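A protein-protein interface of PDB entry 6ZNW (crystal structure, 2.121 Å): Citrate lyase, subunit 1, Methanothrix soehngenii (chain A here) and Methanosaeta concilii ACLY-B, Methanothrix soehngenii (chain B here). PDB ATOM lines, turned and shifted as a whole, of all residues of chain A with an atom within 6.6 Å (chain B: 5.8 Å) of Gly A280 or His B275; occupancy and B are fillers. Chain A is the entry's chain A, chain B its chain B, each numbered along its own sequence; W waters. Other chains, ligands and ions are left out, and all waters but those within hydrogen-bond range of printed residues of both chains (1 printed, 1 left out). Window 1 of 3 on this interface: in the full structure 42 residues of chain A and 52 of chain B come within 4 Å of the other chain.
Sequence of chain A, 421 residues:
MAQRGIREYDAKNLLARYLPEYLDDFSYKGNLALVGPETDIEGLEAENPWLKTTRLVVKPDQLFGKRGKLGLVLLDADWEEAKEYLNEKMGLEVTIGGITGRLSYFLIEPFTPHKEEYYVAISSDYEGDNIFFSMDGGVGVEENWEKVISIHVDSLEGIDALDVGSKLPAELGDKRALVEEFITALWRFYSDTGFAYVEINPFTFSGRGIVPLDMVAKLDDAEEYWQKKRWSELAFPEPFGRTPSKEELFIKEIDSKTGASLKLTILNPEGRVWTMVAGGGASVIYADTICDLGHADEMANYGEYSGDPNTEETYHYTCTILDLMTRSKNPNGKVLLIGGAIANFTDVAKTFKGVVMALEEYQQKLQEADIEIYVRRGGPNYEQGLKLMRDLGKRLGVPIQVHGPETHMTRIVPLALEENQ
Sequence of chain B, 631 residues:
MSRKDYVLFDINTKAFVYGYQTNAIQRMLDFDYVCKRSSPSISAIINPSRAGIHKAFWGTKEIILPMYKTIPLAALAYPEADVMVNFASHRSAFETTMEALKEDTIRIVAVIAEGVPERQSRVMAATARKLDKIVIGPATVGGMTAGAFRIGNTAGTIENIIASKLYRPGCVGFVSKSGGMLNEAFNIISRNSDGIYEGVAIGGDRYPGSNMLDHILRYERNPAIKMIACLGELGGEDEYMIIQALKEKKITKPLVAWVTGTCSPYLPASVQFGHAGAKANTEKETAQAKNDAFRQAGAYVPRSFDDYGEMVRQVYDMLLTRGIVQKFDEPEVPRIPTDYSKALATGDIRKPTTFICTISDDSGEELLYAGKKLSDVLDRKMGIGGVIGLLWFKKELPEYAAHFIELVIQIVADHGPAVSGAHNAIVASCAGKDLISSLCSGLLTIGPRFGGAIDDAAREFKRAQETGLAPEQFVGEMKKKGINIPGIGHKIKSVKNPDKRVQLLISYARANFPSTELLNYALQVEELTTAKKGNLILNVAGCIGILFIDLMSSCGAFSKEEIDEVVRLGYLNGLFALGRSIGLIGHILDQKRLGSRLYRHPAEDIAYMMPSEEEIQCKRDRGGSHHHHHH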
ATOM      1  N   ALA A   2      21.118   6.535   7.798  1.00  0.00           N
ATOM      2  CA  ALA A   2      20.267   6.216   6.659  1.00  0.00           C
ATOM      3  C   ALA A   2      19.696   7.488   6.022  1.00  0.00           C
ATOM      4  O   ALA A   2      19.455   8.479   6.711  1.00  0.00           O
ATOM      5  CB  ALA A   2      19.143   5.285   7.086  1.00  0.00           C
ATOM      6  N   LYS A 263      17.402  -2.497  15.570  1.00  0.00           N
ATOM      7  CA  LYS A 263      16.576  -2.107  14.430  1.00  0.00           C
ATOM      8  C   LYS A 263      15.501  -3.164  14.148  1.00  0.00           C
ATOM      9  O   LYS A 263      15.779  -4.356  14.261  1.00  0.00           O
ATOM     10  CB  LYS A 263      17.468  -1.894  13.190  1.00  0.00           C
ATOM     11  CG  LYS A 263      18.481  -0.775  13.358  1.00  0.00           C
ATOM     12  CD  LYS A 263      19.391  -0.616  12.164  1.00  0.00           C
ATOM     13  CE  LYS A 263      20.272   0.588  12.348  1.00  0.00           C
ATOM     14  NZ  LYS A 263      21.704   0.239  12.164  1.00  0.00           N
ATOM     15  N   VAL A 277      18.382 -11.758  14.458  1.00  0.00           N
ATOM     16  CA  VAL A 277      19.758 -11.979  14.075  1.00  0.00           C
ATOM     17  C   VAL A 277      20.630 -10.835  14.519  1.00  0.00           C
ATOM     18  O   VAL A 277      20.243  -9.673  14.405  1.00  0.00           O
ATOM     19  CB  VAL A 277      19.849 -12.206  12.543  1.00  0.00           C
ATOM     20  CG1 VAL A 277      21.290 -12.467  12.115  1.00  0.00           C
ATOM     21  CG2 VAL A 277      18.946 -13.355  12.119  1.00  0.00           C
ATOM     22  N   ALA A 278      21.816 -11.168  15.028  1.00  0.00           N
ATOM     23  CA  ALA A 278      22.794 -10.191  15.444  1.00  0.00           C
ATOM     24  C   ALA A 278      23.635  -9.717  14.237  1.00  0.00           C
ATOM     25  O   ALA A 278      24.160 -10.535  13.482  1.00  0.00           O
ATOM     26  CB  ALA A 278      23.697 -10.796  16.492  1.00  0.00           C
ATOM     27  N   GLY A 279      23.754  -8.402  14.081  1.00  0.00           N
ATOM     28  CA  GLY A 279      24.567  -7.783  13.045  1.00  0.00           C
ATOM     29  C   GLY A 279      23.845  -7.362  11.778  1.00  0.00           C
ATOM     30  O   GLY A 279      22.902  -8.021  11.343  1.00  0.00           O
ATOM     31  N   GLY A 280      24.313  -6.278  11.169  1.00  0.00           N
ATOM     32  CA  GLY A 280      23.776  -5.774   9.913  1.00  0.00           C
ATOM     33  C   GLY A 280      24.084  -6.734   8.781  1.00  0.00           C
ATOM     34  O   GLY A 280      23.205  -7.059   7.982  1.00  0.00           O
ATOM     35  N   GLY A 281      25.322  -7.224   8.749  1.00  0.00           N
ATOM     36  CA  GLY A 281      25.811  -8.158   7.741  1.00  0.00           C
ATOM     37  C   GLY A 281      25.128  -9.509   7.771  1.00  0.00           C
ATOM     38  O   GLY A 281      24.581  -9.950   6.764  1.00  0.00           O
ATOM     39  N   ALA A 282      25.120 -10.155   8.924  1.00  0.00           N
ATOM     40  CA  ALA A 282      24.503 -11.468   9.085  1.00  0.00           C
ATOM     41  C   ALA A 282      22.980 -11.474   8.896  1.00  0.00           C
ATOM     42  O   ALA A 282      22.454 -12.440   8.353  1.00  0.00           O
ATOM     43  CB  ALA A 282      24.867 -12.057  10.447  1.00  0.00           C
ATOM     44  N   SER A 283      22.275 -10.414   9.322  1.00  0.00           N
ATOM     45  CA  SER A 283      20.816 -10.358   9.204  1.00  0.00           C
ATOM     46  C   SER A 283      20.340 -10.373   7.758  1.00  0.00           C
ATOM     47  O   SER A 283      19.323 -10.996   7.445  1.00  0.00           O
ATOM     48  CB  SER A 283      20.257  -9.158   9.961  1.00  0.00           C
ATOM     49  OG  SER A 283      20.898  -7.952   9.582  1.00  0.00           O
ATOM     50  N   VAL A 284      21.106  -9.708   6.882  1.00  0.00           N
ATOM     51  CA  VAL A 284      20.869  -9.652   5.452  1.00  0.00           C
ATOM     52  C   VAL A 284      21.087 -11.058   4.870  1.00  0.00           C
ATOM     53  O   VAL A 284      20.268 -11.519   4.074  1.00  0.00           O
ATOM     54  CB  VAL A 284      21.793  -8.589   4.797  1.00  0.00           C
ATOM     55  CG1 VAL A 284      21.838  -8.747   3.293  1.00  0.00           C
ATOM     56  CG2 VAL A 284      21.348  -7.182   5.167  1.00  0.00           C
ATOM     57  N   ILE A 285      22.159 -11.752   5.302  1.00  0.00           N
ATOM     58  CA  ILE A 285      22.466 -13.110   4.853  1.00  0.00           C
ATOM     59  C   ILE A 285      21.373 -14.103   5.274  1.00  0.00           C
ATOM     60  O   ILE A 285      20.980 -14.946   4.462  1.00  0.00           O
ATOM     61  CB  ILE A 285      23.884 -13.555   5.273  1.00  0.00           C
ATOM     62  CG1 ILE A 285      24.932 -12.622   4.659  1.00  0.00           C
ATOM     63  CG2 ILE A 285      24.146 -15.002   4.861  1.00  0.00           C
ATOM     64  CD1 ILE A 285      26.308 -12.797   5.175  1.00  0.00           C
ATOM     65  N   TYR A 302      12.395  -7.884   9.132  1.00  0.00           N
ATOM     66  CA  TYR A 302      13.820  -7.704   8.950  1.00  0.00           C
ATOM     67  C   TYR A 302      14.268  -6.932  10.197  1.00  0.00           C
ATOM     68  O   TYR A 302      13.802  -5.819  10.444  1.00  0.00           O
ATOM     69  CB  TYR A 302      14.226  -6.944   7.659  1.00  0.00           C
ATOM     70  CG  TYR A 302      15.697  -6.594   7.721  1.00  0.00           C
ATOM     71  CD1 TYR A 302      16.668  -7.561   7.494  1.00  0.00           C
ATOM     72  CD2 TYR A 302      16.117  -5.367   8.221  1.00  0.00           C
ATOM     73  CE1 TYR A 302      18.016  -7.293   7.698  1.00  0.00           C
ATOM     74  CE2 TYR A 302      17.456  -5.107   8.476  1.00  0.00           C
ATOM     75  CZ  TYR A 302      18.408  -6.061   8.181  1.00  0.00           C
ATOM     76  OH  TYR A 302      19.739  -5.791   8.375  1.00  0.00           O
ATOM     77  N   GLU A 304      17.741  -6.433  13.362  1.00  0.00           N
ATOM     78  CA  GLU A 304      19.121  -6.622  13.810  1.00  0.00           C
ATOM     79  C   GLU A 304      19.400  -5.936  15.117  1.00  0.00           C
ATOM     80  O   GLU A 304      18.833  -4.894  15.425  1.00  0.00           O
ATOM     81  CB  GLU A 304      20.198  -6.251  12.761  1.00  0.00           C
ATOM     82  CG  GLU A 304      20.499  -4.769  12.631  1.00  0.00           C
ATOM     83  CD  GLU A 304      21.800  -4.253  13.212  1.00  0.00           C
ATOM     84  OE1 GLU A 304      22.164  -3.106  12.870  1.00  0.00           O
ATOM     85  OE2 GLU A 304      22.434  -4.953  14.031  1.00  0.00           O
ATOM     86  N   TYR A 305      20.290  -6.550  15.891  1.00  0.00           N
ATOM     87  CA  TYR A 305      20.841  -6.030  17.120  1.00  0.00           C
ATOM     88  C   TYR A 305      22.350  -6.298  17.073  1.00  0.00           C
ATOM     89  O   TYR A 305      22.777  -7.328  16.563  1.00  0.00           O
ATOM     90  CB  TYR A 305      20.171  -6.617  18.383  1.00  0.00           C
ATOM     91  CG  TYR A 305      20.561  -8.045  18.693  1.00  0.00           C
ATOM     92  CD1 TYR A 305      19.964  -9.110  18.031  1.00  0.00           C
ATOM     93  CD2 TYR A 305      21.555  -8.330  19.621  1.00  0.00           C
ATOM     94  CE1 TYR A 305      20.339 -10.422  18.291  1.00  0.00           C
ATOM     95  CE2 TYR A 305      21.944  -9.637  19.882  1.00  0.00           C
ATOM     96  CZ  TYR A 305      21.317 -10.681  19.232  1.00  0.00           C
ATOM     97  OH  TYR A 305      21.689 -11.974  19.486  1.00  0.00           O
ATOM     98  N   SER A 306      23.147  -5.341  17.525  1.00  0.00           N
ATOM     99  CA  SER A 306      24.601  -5.455  17.552  1.00  0.00           C
ATOM    100  C   SER A 306      25.214  -4.313  18.418  1.00  0.00           C
ATOM    101  O   SER A 306      24.467  -3.559  19.044  1.00  0.00           O
ATOM    102  CB  SER A 306      25.178  -5.530  16.132  1.00  0.00           C
ATOM    103  OG  SER A 306      24.857  -4.442  15.285  1.00  0.00           O
ATOM    104  N   GLU B 114      29.213   4.267  15.234  1.00  0.00           N
ATOM    105  CA  GLU B 114      28.077   4.115  14.338  1.00  0.00           C
ATOM    106  C   GLU B 114      27.265   5.409  14.474  1.00  0.00           C
ATOM    107  O   GLU B 114      27.144   5.958  15.578  1.00  0.00           O
ATOM    108  CB  GLU B 114      27.186   2.942  14.780  1.00  0.00           C
ATOM    109  CG  GLU B 114      27.933   1.640  14.990  1.00  0.00           C
ATOM    110  CD  GLU B 114      27.877   0.680  13.820  1.00  0.00           C
ATOM    111  OE1 GLU B 114      26.992   0.854  12.944  1.00  0.00           O
ATOM    112  OE2 GLU B 114      28.722  -0.247  13.775  1.00  0.00           O
ATOM    113  N   LYS B 177      32.434  -5.407   4.469  1.00  0.00           N
ATOM    114  CA  LYS B 177      31.791  -4.193   4.937  1.00  0.00           C
ATOM    115  C   LYS B 177      31.445  -4.418   6.427  1.00  0.00           C
ATOM    116  O   LYS B 177      31.807  -3.624   7.285  1.00  0.00           O
ATOM    117  CB  LYS B 177      30.541  -3.887   4.099  1.00  0.00           C
ATOM    118  CG  LYS B 177      30.857  -2.975   2.928  1.00  0.00           C
ATOM    119  CD  LYS B 177      29.802  -3.039   1.867  1.00  0.00           C
ATOM    120  CE  LYS B 177      30.019  -1.974   0.818  1.00  0.00           C
ATOM    121  NZ  LYS B 177      29.082  -2.157  -0.291  1.00  0.00           N
ATOM    122  N   SER B 178      30.819  -5.557   6.716  1.00  0.00           N
ATOM    123  CA  SER B 178      30.363  -6.002   8.019  1.00  0.00           C
ATOM    124  C   SER B 178      31.488  -6.410   8.992  1.00  0.00           C
ATOM    125  O   SER B 178      32.404  -7.154   8.628  1.00  0.00           O
ATOM    126  CB  SER B 178      29.394  -7.161   7.820  1.00  0.00           C
ATOM    127  OG  SER B 178      28.980  -7.737   9.040  1.00  0.00           O
ATOM    128  N   GLY B 179      31.362  -5.950  10.237  1.00  0.00           N
ATOM    129  CA  GLY B 179      32.292  -6.270  11.318  1.00  0.00           C
ATOM    130  C   GLY B 179      32.103  -7.677  11.853  1.00  0.00           C
ATOM    131  O   GLY B 179      33.075  -8.422  12.006  1.00  0.00           O
ATOM    132  N   GLY B 203      33.349  -1.102   7.289  1.00  0.00           N
ATOM    133  CA  GLY B 203      32.118  -0.564   7.854  1.00  0.00           C
ATOM    134  C   GLY B 203      30.980  -0.604   6.835  1.00  0.00           C
ATOM    135  O   GLY B 203      31.205  -0.856   5.648  1.00  0.00           O
ATOM    136  N   GLY B 204      29.757  -0.356   7.286  1.00  0.00           N
ATOM    137  CA  GLY B 204      28.587  -0.408   6.418  1.00  0.00           C
ATOM    138  C   GLY B 204      28.003   0.932   6.004  1.00  0.00           C
ATOM    139  O   GLY B 204      26.910   0.981   5.431  1.00  0.00           O
ATOM    140  N   ASP B 205      28.711   2.038   6.292  1.00  0.00           N
ATOM    141  CA  ASP B 205      28.233   3.374   5.909  1.00  0.00           C
ATOM    142  C   ASP B 205      28.396   3.556   4.388  1.00  0.00           C
ATOM    143  O   ASP B 205      29.326   2.966   3.815  1.00  0.00           O
ATOM    144  CB  ASP B 205      28.972   4.470   6.701  1.00  0.00           C
ATOM    145  CG  ASP B 205      28.687   4.468   8.197  1.00  0.00           C
ATOM    146  OD1 ASP B 205      27.701   3.813   8.618  1.00  0.00           O
ATOM    147  OD2 ASP B 205      29.437   5.140   8.946  1.00  0.00           O
ATOM    148  N   GLU B 233      27.934  -6.010  -0.043  1.00  0.00           N
ATOM    149  CA  GLU B 233      26.481  -5.960   0.158  1.00  0.00           C
ATOM    150  C   GLU B 233      25.821  -4.938  -0.770  1.00  0.00           C
ATOM    151  O   GLU B 233      26.506  -4.092  -1.334  1.00  0.00           O
ATOM    152  CB  GLU B 233      26.119  -5.687   1.649  1.00  0.00           C
ATOM    153  CG  GLU B 233      26.320  -4.248   2.088  1.00  0.00           C
ATOM    154  CD  GLU B 233      25.866  -3.893   3.492  1.00  0.00           C
ATOM    155  OE1 GLU B 233      25.291  -4.763   4.185  1.00  0.00           O
ATOM    156  OE2 GLU B 233      26.095  -2.731   3.899  1.00  0.00           O
ATOM    157  N   GLN B 272      15.025  -0.349   4.322  1.00  0.00           N
ATOM    158  CA  GLN B 272      16.386   0.073   4.622  1.00  0.00           C
ATOM    159  C   GLN B 272      16.952  -1.040   5.507  1.00  0.00           C
ATOM    160  O   GLN B 272      16.306  -1.425   6.484  1.00  0.00           O
ATOM    161  CB  GLN B 272      16.374   1.425   5.368  1.00  0.00           C
ATOM    162  CG  GLN B 272      17.693   1.814   6.046  1.00  0.00           C
ATOM    163  CD  GLN B 272      18.789   2.155   5.071  1.00  0.00           C
ATOM    164  OE1 GLN B 272      18.628   3.003   4.182  1.00  0.00           O
ATOM    165  NE2 GLN B 272      19.932   1.505   5.220  1.00  0.00           N
ATOM    166  N   PHE B 273      18.105  -1.604   5.133  1.00  0.00           N
ATOM    167  CA  PHE B 273      18.699  -2.681   5.914  1.00  0.00           C
ATOM    168  C   PHE B 273      19.618  -2.116   7.024  1.00  0.00           C
ATOM    169  O   PHE B 273      19.783  -0.897   7.118  1.00  0.00           O
ATOM    170  CB  PHE B 273      19.367  -3.726   5.001  1.00  0.00           C
ATOM    171  CG  PHE B 273      18.364  -4.396   4.083  1.00  0.00           C
ATOM    172  CD1 PHE B 273      17.556  -5.422   4.539  1.00  0.00           C
ATOM    173  CD2 PHE B 273      18.205  -3.970   2.769  1.00  0.00           C
ATOM    174  CE1 PHE B 273      16.619  -6.019   3.694  1.00  0.00           C
ATOM    175  CE2 PHE B 273      17.268  -4.569   1.931  1.00  0.00           C
ATOM    176  CZ  PHE B 273      16.484  -5.591   2.396  1.00  0.00           C
ATOM    177  N   GLY B 274      20.115  -2.999   7.901  1.00  0.00           N
ATOM    178  CA  GLY B 274      20.944  -2.683   9.059  1.00  0.00           C
ATOM    179  C   GLY B 274      21.978  -1.598   8.862  1.00  0.00           C
ATOM    180  O   GLY B 274      21.891  -0.547   9.496  1.00  0.00           O
ATOM    181  N   HIS B 275      22.950  -1.834   7.979  1.00  0.00           N
ATOM    182  CA  HIS B 275      23.986  -0.847   7.698  1.00  0.00           C
ATOM    183  C   HIS B 275      23.388   0.410   7.062  1.00  0.00           C
ATOM    184  O   HIS B 275      22.450   0.306   6.267  1.00  0.00           O
ATOM    185  CB  HIS B 275      25.063  -1.448   6.786  1.00  0.00           C
ATOM    186  CG  HIS B 275      25.850  -2.557   7.418  1.00  0.00           C
ATOM    187  ND1 HIS B 275      26.490  -3.515   6.653  1.00  0.00           N
ATOM    188  CD2 HIS B 275      26.079  -2.823   8.725  1.00  0.00           C
ATOM    189  CE1 HIS B 275      27.078  -4.331   7.509  1.00  0.00           C
ATOM    190  NE2 HIS B 275      26.861  -3.954   8.770  1.00  0.00           N
ATOM    191  N   ALA B 276      23.917   1.597   7.403  1.00  0.00           N
ATOM    192  CA  ALA B 276      23.414   2.864   6.869  1.00  0.00           C
ATOM    193  C   ALA B 276      23.413   2.897   5.342  1.00  0.00           C
ATOM    194  O   ALA B 276      22.479   3.421   4.747  1.00  0.00           O
ATOM    195  CB  ALA B 276      24.212   4.033   7.423  1.00  0.00           C
ATOM    196  N   GLY B 277      24.407   2.272   4.725  1.00  0.00           N
ATOM    197  CA  GLY B 277      24.504   2.231   3.273  1.00  0.00           C
ATOM    198  C   GLY B 277      23.835   1.056   2.585  1.00  0.00           C
ATOM    199  O   GLY B 277      23.890   0.956   1.357  1.00  0.00           O
ATOM    200  N   ALA B 278      23.207   0.147   3.355  1.00  0.00           N
ATOM    201  CA  ALA B 278      22.557  -1.030   2.774  1.00  0.00           C
ATOM    202  C   ALA B 278      21.130  -0.777   2.273  1.00  0.00           C
ATOM    203  O   ALA B 278      20.164  -1.272   2.843  1.00  0.00           O
ATOM    204  CB  ALA B 278      22.590  -2.203   3.742  1.00  0.00           C
ATOM    205  N   LYS B 279      21.009  -0.009   1.199  1.00  0.00           N
ATOM    206  CA  LYS B 279      19.735   0.260   0.542  1.00  0.00           C
ATOM    207  C   LYS B 279      19.987   0.538  -0.931  1.00  0.00           C
ATOM    208  O   LYS B 279      20.565   1.570  -1.272  1.00  0.00           O
ATOM    209  CB  LYS B 279      18.951   1.416   1.186  1.00  0.00           C
ATOM    210  CG  LYS B 279      17.505   1.457   0.678  1.00  0.00           C
ATOM    211  CD  LYS B 279      16.740   2.689   1.122  1.00  0.00           C
ATOM    212  CE  LYS B 279      15.265   2.541   0.830  1.00  0.00           C
ATOM    213  NZ  LYS B 279      14.600   3.858   0.665  1.00  0.00           N
HETATM  214  O   HOH W   1      27.113  -9.500  11.287  1.00  0.00           O
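OH of Tyr A302 sits at hydrogen-bond distance from N of Gly B274.
The side-chain amino group of Lys A263 lies within hydrogen-bond range of the backbone carbonyl oxygen of Gly B274 (2.8 Å).
O of Ala B276 lies within hydrogen-bond range of NE2 of Gln B272, at 3.2 Å.
OE1 of Glu A304 is in salt-bridge range of NZ of Lys A263.
The backbone carbonyl oxygen of Ala B278 sits at hydrogen-bond distance from the backbone NH of Phe B273 (3.1 Å).
The side-chain hydroxyl (OG) of Ser A283 lies within hydrogen-bond range of the backbone carbonyl oxygen (O) of Gly A280.
The side-chain carboxylate (OE2) of Glu B233 sits at hydrogen-bond distance from a ring nitrogen (ND1) of His B275 (2.9 Å).
The side-chain hydroxyl of Ser A283 sits at hydrogen-bond distance from the side-chain hydroxyl of Tyr A302 (2.7 Å).
Among the printed residues, pairs that only touch across the chains: Ala A2 with Gln B272 (3.7 Å), Ala A2 with Ala B276 (3.997 Å), Gly A280 with His B275 (3.8 Å), Gly A281 with Ser B178 (3.5 Å), Gly A281 with His B275 (3.6 Å), Val A284 with Phe B273 (3.99 Å) and Tyr A302 with Phe B273 (3.7 Å).
Printed residues of chain A within 4 Å of Phe B273: Val A284 (3.99 Å) and Tyr A302 (3.7 Å).
Of the printed residues of chain B, Gly A281 touches Ser B178 and His B275.
Hydrophobic or aromatic side chains of chain A that line the printed part of chain B: Ala A2, Val A284 and Tyr A302.
Of the 16 printed residues of chain B, 6 touch a printed residue of chain A.
Printed residues of chain B that touch a printed residue of chain A: Ser B178, Gln B272, Phe B273, Gly B274, His B275 and Ala B276.
Among the printed residues, 9 pairs touch across the chains.
Water W1 lies within hydrogen-bond range of the backbone NH of Ala A282 (3.2 Å) and the side-chain hydroxyl of Ser B178 (3.4 Å).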
